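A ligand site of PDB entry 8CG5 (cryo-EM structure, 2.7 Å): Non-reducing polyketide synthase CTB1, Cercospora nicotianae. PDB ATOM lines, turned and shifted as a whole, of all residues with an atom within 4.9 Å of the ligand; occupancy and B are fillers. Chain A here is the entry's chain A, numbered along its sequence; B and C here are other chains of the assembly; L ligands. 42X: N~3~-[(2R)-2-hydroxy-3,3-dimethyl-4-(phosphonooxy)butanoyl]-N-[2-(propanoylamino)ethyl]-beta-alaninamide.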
ATOM      1  N   CYS A 553      29.866  21.402 -25.106  1.00  0.00           N
ATOM      2  CA  CYS A 553      30.015  22.336 -24.000  1.00  0.00           C
ATOM      3  C   CYS A 553      31.487  22.658 -23.742  1.00  0.00           C
ATOM      4  O   CYS A 553      31.808  23.516 -22.917  1.00  0.00           O
ATOM      5  CB  CYS A 553      29.383  21.769 -22.727  1.00  0.00           C
ATOM      6  SG  CYS A 553      27.742  22.397 -22.348  1.00  0.00           S
ATOM      7  N   LEU A 592      17.084  21.672 -22.182  1.00  0.00           N
ATOM      8  CA  LEU A 592      18.071  21.332 -21.175  1.00  0.00           C
ATOM      9  C   LEU A 592      17.418  21.004 -19.843  1.00  0.00           C
ATOM     10  O   LEU A 592      17.917  20.152 -19.109  1.00  0.00           O
ATOM     11  CB  LEU A 592      19.069  22.479 -21.012  1.00  0.00           C
ATOM     12  CG  LEU A 592      20.201  22.514 -22.039  1.00  0.00           C
ATOM     13  CD1 LEU A 592      20.732  23.921 -22.204  1.00  0.00           C
ATOM     14  CD2 LEU A 592      21.319  21.562 -21.632  1.00  0.00           C
ATOM     15  N   GLY A 595      15.892  17.482 -20.031  1.00  0.00           N
ATOM     16  CA  GLY A 595      16.915  16.484 -19.846  1.00  0.00           C
ATOM     17  C   GLY A 595      17.503  16.455 -18.452  1.00  0.00           C
ATOM     18  O   GLY A 595      18.482  15.734 -18.225  1.00  0.00           O
ATOM     19  N   HIS A 596      16.955  17.231 -17.515  1.00  0.00           N
ATOM     20  CA  HIS A 596      17.456  17.277 -16.154  1.00  0.00           C
ATOM     21  C   HIS A 596      18.925  17.717 -16.118  1.00  0.00           C
ATOM     22  O   HIS A 596      19.731  17.190 -15.350  1.00  0.00           O
ATOM     23  CB  HIS A 596      17.287  15.931 -15.444  1.00  0.00           C
ATOM     24  CG  HIS A 596      15.884  15.423 -15.476  1.00  0.00           C
ATOM     25  ND1 HIS A 596      15.518  14.266 -16.141  1.00  0.00           N
ATOM     26  CD2 HIS A 596      14.741  15.907 -14.933  1.00  0.00           C
ATOM     27  CE1 HIS A 596      14.228  14.059 -15.994  1.00  0.00           C
ATOM     28  NE2 HIS A 596      13.731  15.042 -15.265  1.00  0.00           N
ATOM     29  N   PHE A 597      19.264  18.689 -16.961  1.00  0.00           N
ATOM     30  CA  PHE A 597      20.615  19.245 -16.974  1.00  0.00           C
ATOM     31  C   PHE A 597      20.739  20.455 -16.057  1.00  0.00           C
ATOM     32  O   PHE A 597      21.784  20.641 -15.424  1.00  0.00           O
ATOM     33  CB  PHE A 597      21.012  19.641 -18.392  1.00  0.00           C
ATOM     34  CG  PHE A 597      21.262  18.483 -19.307  1.00  0.00           C
ATOM     35  CD1 PHE A 597      22.414  17.738 -19.207  1.00  0.00           C
ATOM     36  CD2 PHE A 597      20.338  18.145 -20.285  1.00  0.00           C
ATOM     37  CE1 PHE A 597      22.649  16.672 -20.045  1.00  0.00           C
ATOM     38  CE2 PHE A 597      20.562  17.082 -21.132  1.00  0.00           C
ATOM     39  CZ  PHE A 597      21.718  16.345 -21.012  1.00  0.00           C
ATOM     40  N   TYR A 614      23.317  22.556 -13.237  1.00  0.00           N
ATOM     41  CA  TYR A 614      24.130  23.745 -13.487  1.00  0.00           C
ATOM     42  C   TYR A 614      23.248  24.883 -13.998  1.00  0.00           C
ATOM     43  O   TYR A 614      22.065  24.698 -14.285  1.00  0.00           O
ATOM     44  CB  TYR A 614      25.252  23.440 -14.488  1.00  0.00           C
ATOM     45  CG  TYR A 614      24.860  23.394 -15.944  1.00  0.00           C
ATOM     46  CD1 TYR A 614      24.716  24.561 -16.687  1.00  0.00           C
ATOM     47  CD2 TYR A 614      24.669  22.193 -16.597  1.00  0.00           C
ATOM     48  CE1 TYR A 614      24.374  24.525 -18.013  1.00  0.00           C
ATOM     49  CE2 TYR A 614      24.324  22.148 -17.933  1.00  0.00           C
ATOM     50  CZ  TYR A 614      24.181  23.313 -18.637  1.00  0.00           C
ATOM     51  OH  TYR A 614      23.841  23.287 -19.962  1.00  0.00           O
ATOM     52  N   SER A 655      26.297   5.857 -19.935  1.00  0.00           N
ATOM     53  CA  SER A 655      25.385   6.534 -20.850  1.00  0.00           C
ATOM     54  C   SER A 655      26.164   7.599 -21.610  1.00  0.00           C
ATOM     55  O   SER A 655      27.251   8.006 -21.213  1.00  0.00           O
ATOM     56  CB  SER A 655      24.216   7.166 -20.105  1.00  0.00           C
ATOM     57  OG  SER A 655      23.739   8.309 -20.789  1.00  0.00           O
ATOM     58  N   THR A 657      25.658  10.792 -22.133  1.00  0.00           N
ATOM     59  CA  THR A 657      25.877  12.053 -21.417  1.00  0.00           C
ATOM     60  C   THR A 657      26.709  11.870 -20.162  1.00  0.00           C
ATOM     61  O   THR A 657      27.382  12.810 -19.724  1.00  0.00           O
ATOM     62  CB  THR A 657      24.535  12.691 -21.057  1.00  0.00           C
ATOM     63  OG1 THR A 657      23.702  11.720 -20.419  1.00  0.00           O
ATOM     64  CG2 THR A 657      23.838  13.212 -22.301  1.00  0.00           C
ATOM     65  N   ARG A 658      26.686  10.681 -19.566  1.00  0.00           N
ATOM     66  CA  ARG A 658      27.377  10.469 -18.299  1.00  0.00           C
ATOM     67  C   ARG A 658      28.887  10.533 -18.503  1.00  0.00           C
ATOM     68  O   ARG A 658      29.399  10.050 -19.518  1.00  0.00           O
ATOM     69  CB  ARG A 658      26.983   9.114 -17.713  1.00  0.00           C
ATOM     70  CG  ARG A 658      27.657   8.781 -16.405  1.00  0.00           C
ATOM     71  CD  ARG A 658      27.022   7.565 -15.771  1.00  0.00           C
ATOM     72  NE  ARG A 658      25.843   7.898 -14.987  1.00  0.00           N
ATOM     73  CZ  ARG A 658      25.175   7.033 -14.236  1.00  0.00           C
ATOM     74  NH1 ARG A 658      25.520   5.767 -14.169  1.00  0.00           N
ATOM     75  NH2 ARG A 658      24.117   7.456 -13.550  1.00  0.00           N
ATOM     76  N   PRO A 659      29.626  11.136 -17.570  1.00  0.00           N
ATOM     77  CA  PRO A 659      31.088  11.155 -17.685  1.00  0.00           C
ATOM     78  C   PRO A 659      31.712   9.804 -17.372  1.00  0.00           C
ATOM     79  O   PRO A 659      31.049   8.856 -16.949  1.00  0.00           O
ATOM     80  CB  PRO A 659      31.479  12.208 -16.638  1.00  0.00           C
ATOM     81  CG  PRO A 659      30.350  12.072 -15.659  1.00  0.00           C
ATOM     82  CD  PRO A 659      29.226  12.174 -16.609  1.00  0.00           C
ATOM     83  N   HIS A 688      36.395  21.556 -14.308  1.00  0.00           N
ATOM     84  CA  HIS A 688      35.112  21.831 -14.939  1.00  0.00           C
ATOM     85  C   HIS A 688      34.053  22.179 -13.887  1.00  0.00           C
ATOM     86  O   HIS A 688      33.394  23.214 -13.972  1.00  0.00           O
ATOM     87  CB  HIS A 688      34.675  20.631 -15.775  1.00  0.00           C
ATOM     88  CG  HIS A 688      33.589  20.942 -16.761  1.00  0.00           C
ATOM     89  ND1 HIS A 688      33.704  21.946 -17.705  1.00  0.00           N
ATOM     90  CD2 HIS A 688      32.370  20.379 -16.964  1.00  0.00           C
ATOM     91  CE1 HIS A 688      32.606  21.986 -18.440  1.00  0.00           C
ATOM     92  NE2 HIS A 688      31.781  21.046 -18.000  1.00  0.00           N
ATOM     93  N   THR A 690      30.869  21.408 -12.809  1.00  0.00           N
ATOM     94  CA  THR A 690      29.611  21.899 -13.355  1.00  0.00           C
ATOM     95  C   THR A 690      28.451  21.801 -12.372  1.00  0.00           C
ATOM     96  O   THR A 690      27.293  21.948 -12.776  1.00  0.00           O
ATOM     97  CB  THR A 690      29.274  21.157 -14.642  1.00  0.00           C
ATOM     98  OG1 THR A 690      28.455  21.981 -15.479  1.00  0.00           O
ATOM     99  CG2 THR A 690      28.548  19.852 -14.353  1.00  0.00           C
ATOM    100  N   THR A 692      27.149  19.204 -10.504  1.00  0.00           N
ATOM    101  CA  THR A 692      26.342  17.998 -10.475  1.00  0.00           C
ATOM    102  C   THR A 692      27.021  16.967  -9.579  1.00  0.00           C
ATOM    103  O   THR A 692      28.244  16.833  -9.618  1.00  0.00           O
ATOM    104  CB  THR A 692      26.129  17.409 -11.876  1.00  0.00           C
ATOM    105  OG1 THR A 692      27.341  16.809 -12.339  1.00  0.00           O
ATOM    106  CG2 THR A 692      25.672  18.483 -12.856  1.00  0.00           C
ATOM    107  N   HIS A 733      27.723  28.458 -16.118  1.00  0.00           N
ATOM    108  CA  HIS A 733      28.324  27.623 -17.151  1.00  0.00           C
ATOM    109  C   HIS A 733      28.105  28.311 -18.498  1.00  0.00           C
ATOM    110  O   HIS A 733      27.024  28.224 -19.082  1.00  0.00           O
ATOM    111  CB  HIS A 733      27.726  26.221 -17.133  1.00  0.00           C
ATOM    112  CG  HIS A 733      28.515  25.221 -17.913  1.00  0.00           C
ATOM    113  ND1 HIS A 733      28.146  23.894 -18.008  1.00  0.00           N
ATOM    114  CD2 HIS A 733      29.641  25.342 -18.653  1.00  0.00           C
ATOM    115  CE1 HIS A 733      29.012  23.244 -18.755  1.00  0.00           C
ATOM    116  NE2 HIS A 733      29.933  24.106 -19.163  1.00  0.00           N
ATOM    117  N   GLU A 735      29.176  27.375 -21.178  1.00  0.00           N
ATOM    118  CA  GLU A 735      28.769  26.193 -21.933  1.00  0.00           C
ATOM    119  C   GLU A 735      29.211  26.231 -23.389  1.00  0.00           C
ATOM    120  O   GLU A 735      29.027  25.238 -24.088  1.00  0.00           O
ATOM    121  CB  GLU A 735      27.261  25.951 -21.853  1.00  0.00           C
ATOM    122  CG  GLU A 735      26.451  26.384 -23.060  1.00  0.00           C
ATOM    123  CD  GLU A 735      24.968  26.371 -22.783  1.00  0.00           C
ATOM    124  OE1 GLU A 735      24.565  25.814 -21.737  1.00  0.00           O
ATOM    125  OE2 GLU A 735      24.194  26.914 -23.591  1.00  0.00           O
ATOM    126  N   SER A 802      32.448  17.589 -21.644  1.00  0.00           N
ATOM    127  CA  SER A 802      31.374  17.730 -22.603  1.00  0.00           C
ATOM    128  C   SER A 802      30.211  16.818 -22.251  1.00  0.00           C
ATOM    129  O   SER A 802      30.386  15.765 -21.651  1.00  0.00           O
ATOM    130  CB  SER A 802      31.858  17.382 -24.008  1.00  0.00           C
ATOM    131  OG  SER A 802      30.755  17.174 -24.871  1.00  0.00           O
ATOM    132  N   ALA A 803      29.011  17.263 -22.652  1.00  0.00           N
ATOM    133  CA  ALA A 803      27.851  16.380 -22.599  1.00  0.00           C
ATOM    134  C   ALA A 803      27.945  15.291 -23.664  1.00  0.00           C
ATOM    135  O   ALA A 803      27.458  14.179 -23.449  1.00  0.00           O
ATOM    136  CB  ALA A 803      26.564  17.184 -22.780  1.00  0.00           C
ATOM    137  N   SER B  46      20.315   6.466 -18.657  1.00  0.00           N
ATOM    138  CA  SER B  46      19.989   7.019 -17.352  1.00  0.00           C
ATOM    139  C   SER B  46      19.031   8.193 -17.497  1.00  0.00           C
ATOM    140  O   SER B  46      18.169   8.412 -16.641  1.00  0.00           O
ATOM    141  CB  SER B  46      21.266   7.462 -16.629  1.00  0.00           C
ATOM    142  OG  SER B  46      21.589   8.805 -16.932  1.00  0.00           O
ATOM    143  N   LEU B  47      19.157   8.936 -18.601  1.00  0.00           N
ATOM    144  CA  LEU B  47      18.277  10.066 -18.842  1.00  0.00           C
ATOM    145  C   LEU B  47      16.819   9.636 -18.917  1.00  0.00           C
ATOM    146  O   LEU B  47      15.933  10.282 -18.340  1.00  0.00           O
ATOM    147  CB  LEU B  47      18.693  10.770 -20.138  1.00  0.00           C
ATOM    148  CG  LEU B  47      17.952  12.069 -20.471  1.00  0.00           C
ATOM    149  CD1 LEU B  47      18.203  13.093 -19.401  1.00  0.00           C
ATOM    150  CD2 LEU B  47      18.370  12.580 -21.831  1.00  0.00           C
ATOM    151  N   LEU B  50      15.462   8.122 -15.563  1.00  0.00           N
ATOM    152  CA  LEU B  50      15.029   9.159 -14.631  1.00  0.00           C
ATOM    153  C   LEU B  50      13.572   9.523 -14.849  1.00  0.00           C
ATOM    154  O   LEU B  50      12.808   9.659 -13.892  1.00  0.00           O
ATOM    155  CB  LEU B  50      15.911  10.395 -14.760  1.00  0.00           C
ATOM    156  CG  LEU B  50      17.330  10.265 -14.182  1.00  0.00           C
ATOM    157  CD1 LEU B  50      18.215  11.381 -14.701  1.00  0.00           C
ATOM    158  CD2 LEU B  50      17.291  10.259 -12.667  1.00  0.00           C
ATOM    159  N   PHE B  70      18.164   1.260 -14.865  1.00  0.00           N
ATOM    160  CA  PHE B  70      19.140   0.622 -15.745  1.00  0.00           C
ATOM    161  C   PHE B  70      20.391   0.192 -14.993  1.00  0.00           C
ATOM    162  O   PHE B  70      21.065  -0.762 -15.415  1.00  0.00           O
ATOM    163  CB  PHE B  70      19.501   1.577 -16.881  1.00  0.00           C
ATOM    164  CG  PHE B  70      20.615   2.529 -16.546  1.00  0.00           C
ATOM    165  CD1 PHE B  70      20.371   3.653 -15.764  1.00  0.00           C
ATOM    166  CD2 PHE B  70      21.908   2.301 -16.995  1.00  0.00           C
ATOM    167  CE1 PHE B  70      21.391   4.516 -15.453  1.00  0.00           C
ATOM    168  CE2 PHE B  70      22.930   3.174 -16.683  1.00  0.00           C
ATOM    169  CZ  PHE B  70      22.671   4.282 -15.912  1.00  0.00           C
ATOM    170  N   ILE C 524      18.122  17.852 -26.736  1.00  0.00           N
ATOM    171  CA  ILE C 524      19.522  18.287 -26.839  1.00  0.00           C
ATOM    172  C   ILE C 524      20.372  17.154 -27.400  1.00  0.00           C
ATOM    173  O   ILE C 524      21.050  17.352 -28.411  1.00  0.00           O
ATOM    174  CB  ILE C 524      20.049  18.781 -25.486  1.00  0.00           C
ATOM    175  CG1 ILE C 524      19.280  20.014 -25.021  1.00  0.00           C
ATOM    176  CG2 ILE C 524      21.534  19.102 -25.580  1.00  0.00           C
ATOM    177  CD1 ILE C 524      19.277  21.172 -25.990  1.00  0.00           C
HETATM  178  C14 42X L   1      23.169  13.713 -18.090  1.00  0.00           C
HETATM  179  C10 42X L   1      21.709  14.172 -16.124  1.00  0.00           C
HETATM  180  O01 42X L   1      23.840   9.406 -15.827  1.00  0.00           O
HETATM  181  P02 42X L   1      22.344   9.580 -15.686  1.00  0.00           P
HETATM  182  O03 42X L   1      21.904   9.025 -14.358  1.00  0.00           O
HETATM  183  O05 42X L   1      21.969  11.182 -15.728  1.00  0.00           O
HETATM  184  C06 42X L   1      22.041  11.852 -16.945  1.00  0.00           C
HETATM  185  C09 42X L   1      22.720  13.198 -16.729  1.00  0.00           C
HETATM  186  C18 42X L   1      23.894  13.001 -15.767  1.00  0.00           C
HETATM  187  O20 42X L   1      24.382  11.695 -15.938  1.00  0.00           O
HETATM  188  C22 42X L   1      25.045  13.973 -16.034  1.00  0.00           C
HETATM  189  O23 42X L   1      26.145  13.551 -16.100  1.00  0.00           O
HETATM  190  N24 42X L   1      24.803  15.387 -16.224  1.00  0.00           N
HETATM  191  C26 42X L   1      25.933  16.270 -16.477  1.00  0.00           C
HETATM  192  C29 42X L   1      26.603  15.817 -17.765  1.00  0.00           C
HETATM  193  C32 42X L   1      27.103  17.015 -18.566  1.00  0.00           C
HETATM  194  O33 42X L   1      26.959  17.043 -19.733  1.00  0.00           O
HETATM  195  N34 42X L   1      27.758  18.130 -17.894  1.00  0.00           N
HETATM  196  C36 42X L   1      28.232  19.262 -18.679  1.00  0.00           C
HETATM  197  C39 42X L   1      27.050  19.997 -19.311  1.00  0.00           C
HETATM  198  N42 42X L   1      27.398  20.350 -20.670  1.00  0.00           N
HETATM  199  C44 42X L   1      26.355  20.740 -21.602  1.00  0.00           C
HETATM  200  O45 42X L   1      25.225  20.769 -21.253  1.00  0.00           O
HETATM  201  C46 42X L   1      26.706  21.119 -23.040  1.00  0.00           C
HETATM  202  C49 42X L   1      25.447  21.411 -23.871  1.00  0.00           C
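His 596 touches the ligand. Phe 597 touches the ligand. Thr 657 touches the ligand. Pro 659 touches the ligand (CD to O23, 3.4 Å). His 733 touches the ligand. CA of Ala 803 touches O33 of the ligand (3.1 Å). Leu 50 of chain B touches the ligand. 11 residues have an atom within 4 Å of the ligand: Cys 553, His 596, Phe 597, Tyr 614, Thr 657, Arg 658, Pro 659, His 733, Ala 803, Ser 46 of chain B and Leu 50 of chain B. The nearest printed residue that does not touch the ligand is Leu 592 (4.004 Å).
OG of Ser 46 of chain B is bonded to P02 of the ligand (1.7 Å). SG of Cys 553 is covalently linked to C46 of the ligand (1.8 Å). NE of Arg 658 is in salt-bridge range of O01 of the ligand, at 2.6 Å. O45 of the ligand sits at hydrogen-bond distance from OH of Tyr 614, 3.1 Å away.
The side-chain hydroxyl of Ser 655 sits close to the backbone NH of Thr 657 (3.4 Å). The backbone NH of Tyr 614 lies within hydrogen-bond range of the backbone carbonyl oxygen of Phe 597 (3.3 Å). OH of Tyr 614 sits at hydrogen-bond distance from OE1 of Glu 735 (3.2 Å). O of Leu 592 is in hydrogen-bond range of N of Phe 597, at 2.9 Å. ND1 of His 733 is in hydrogen-bond range of OG1 of Thr 690 (3.2 Å).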
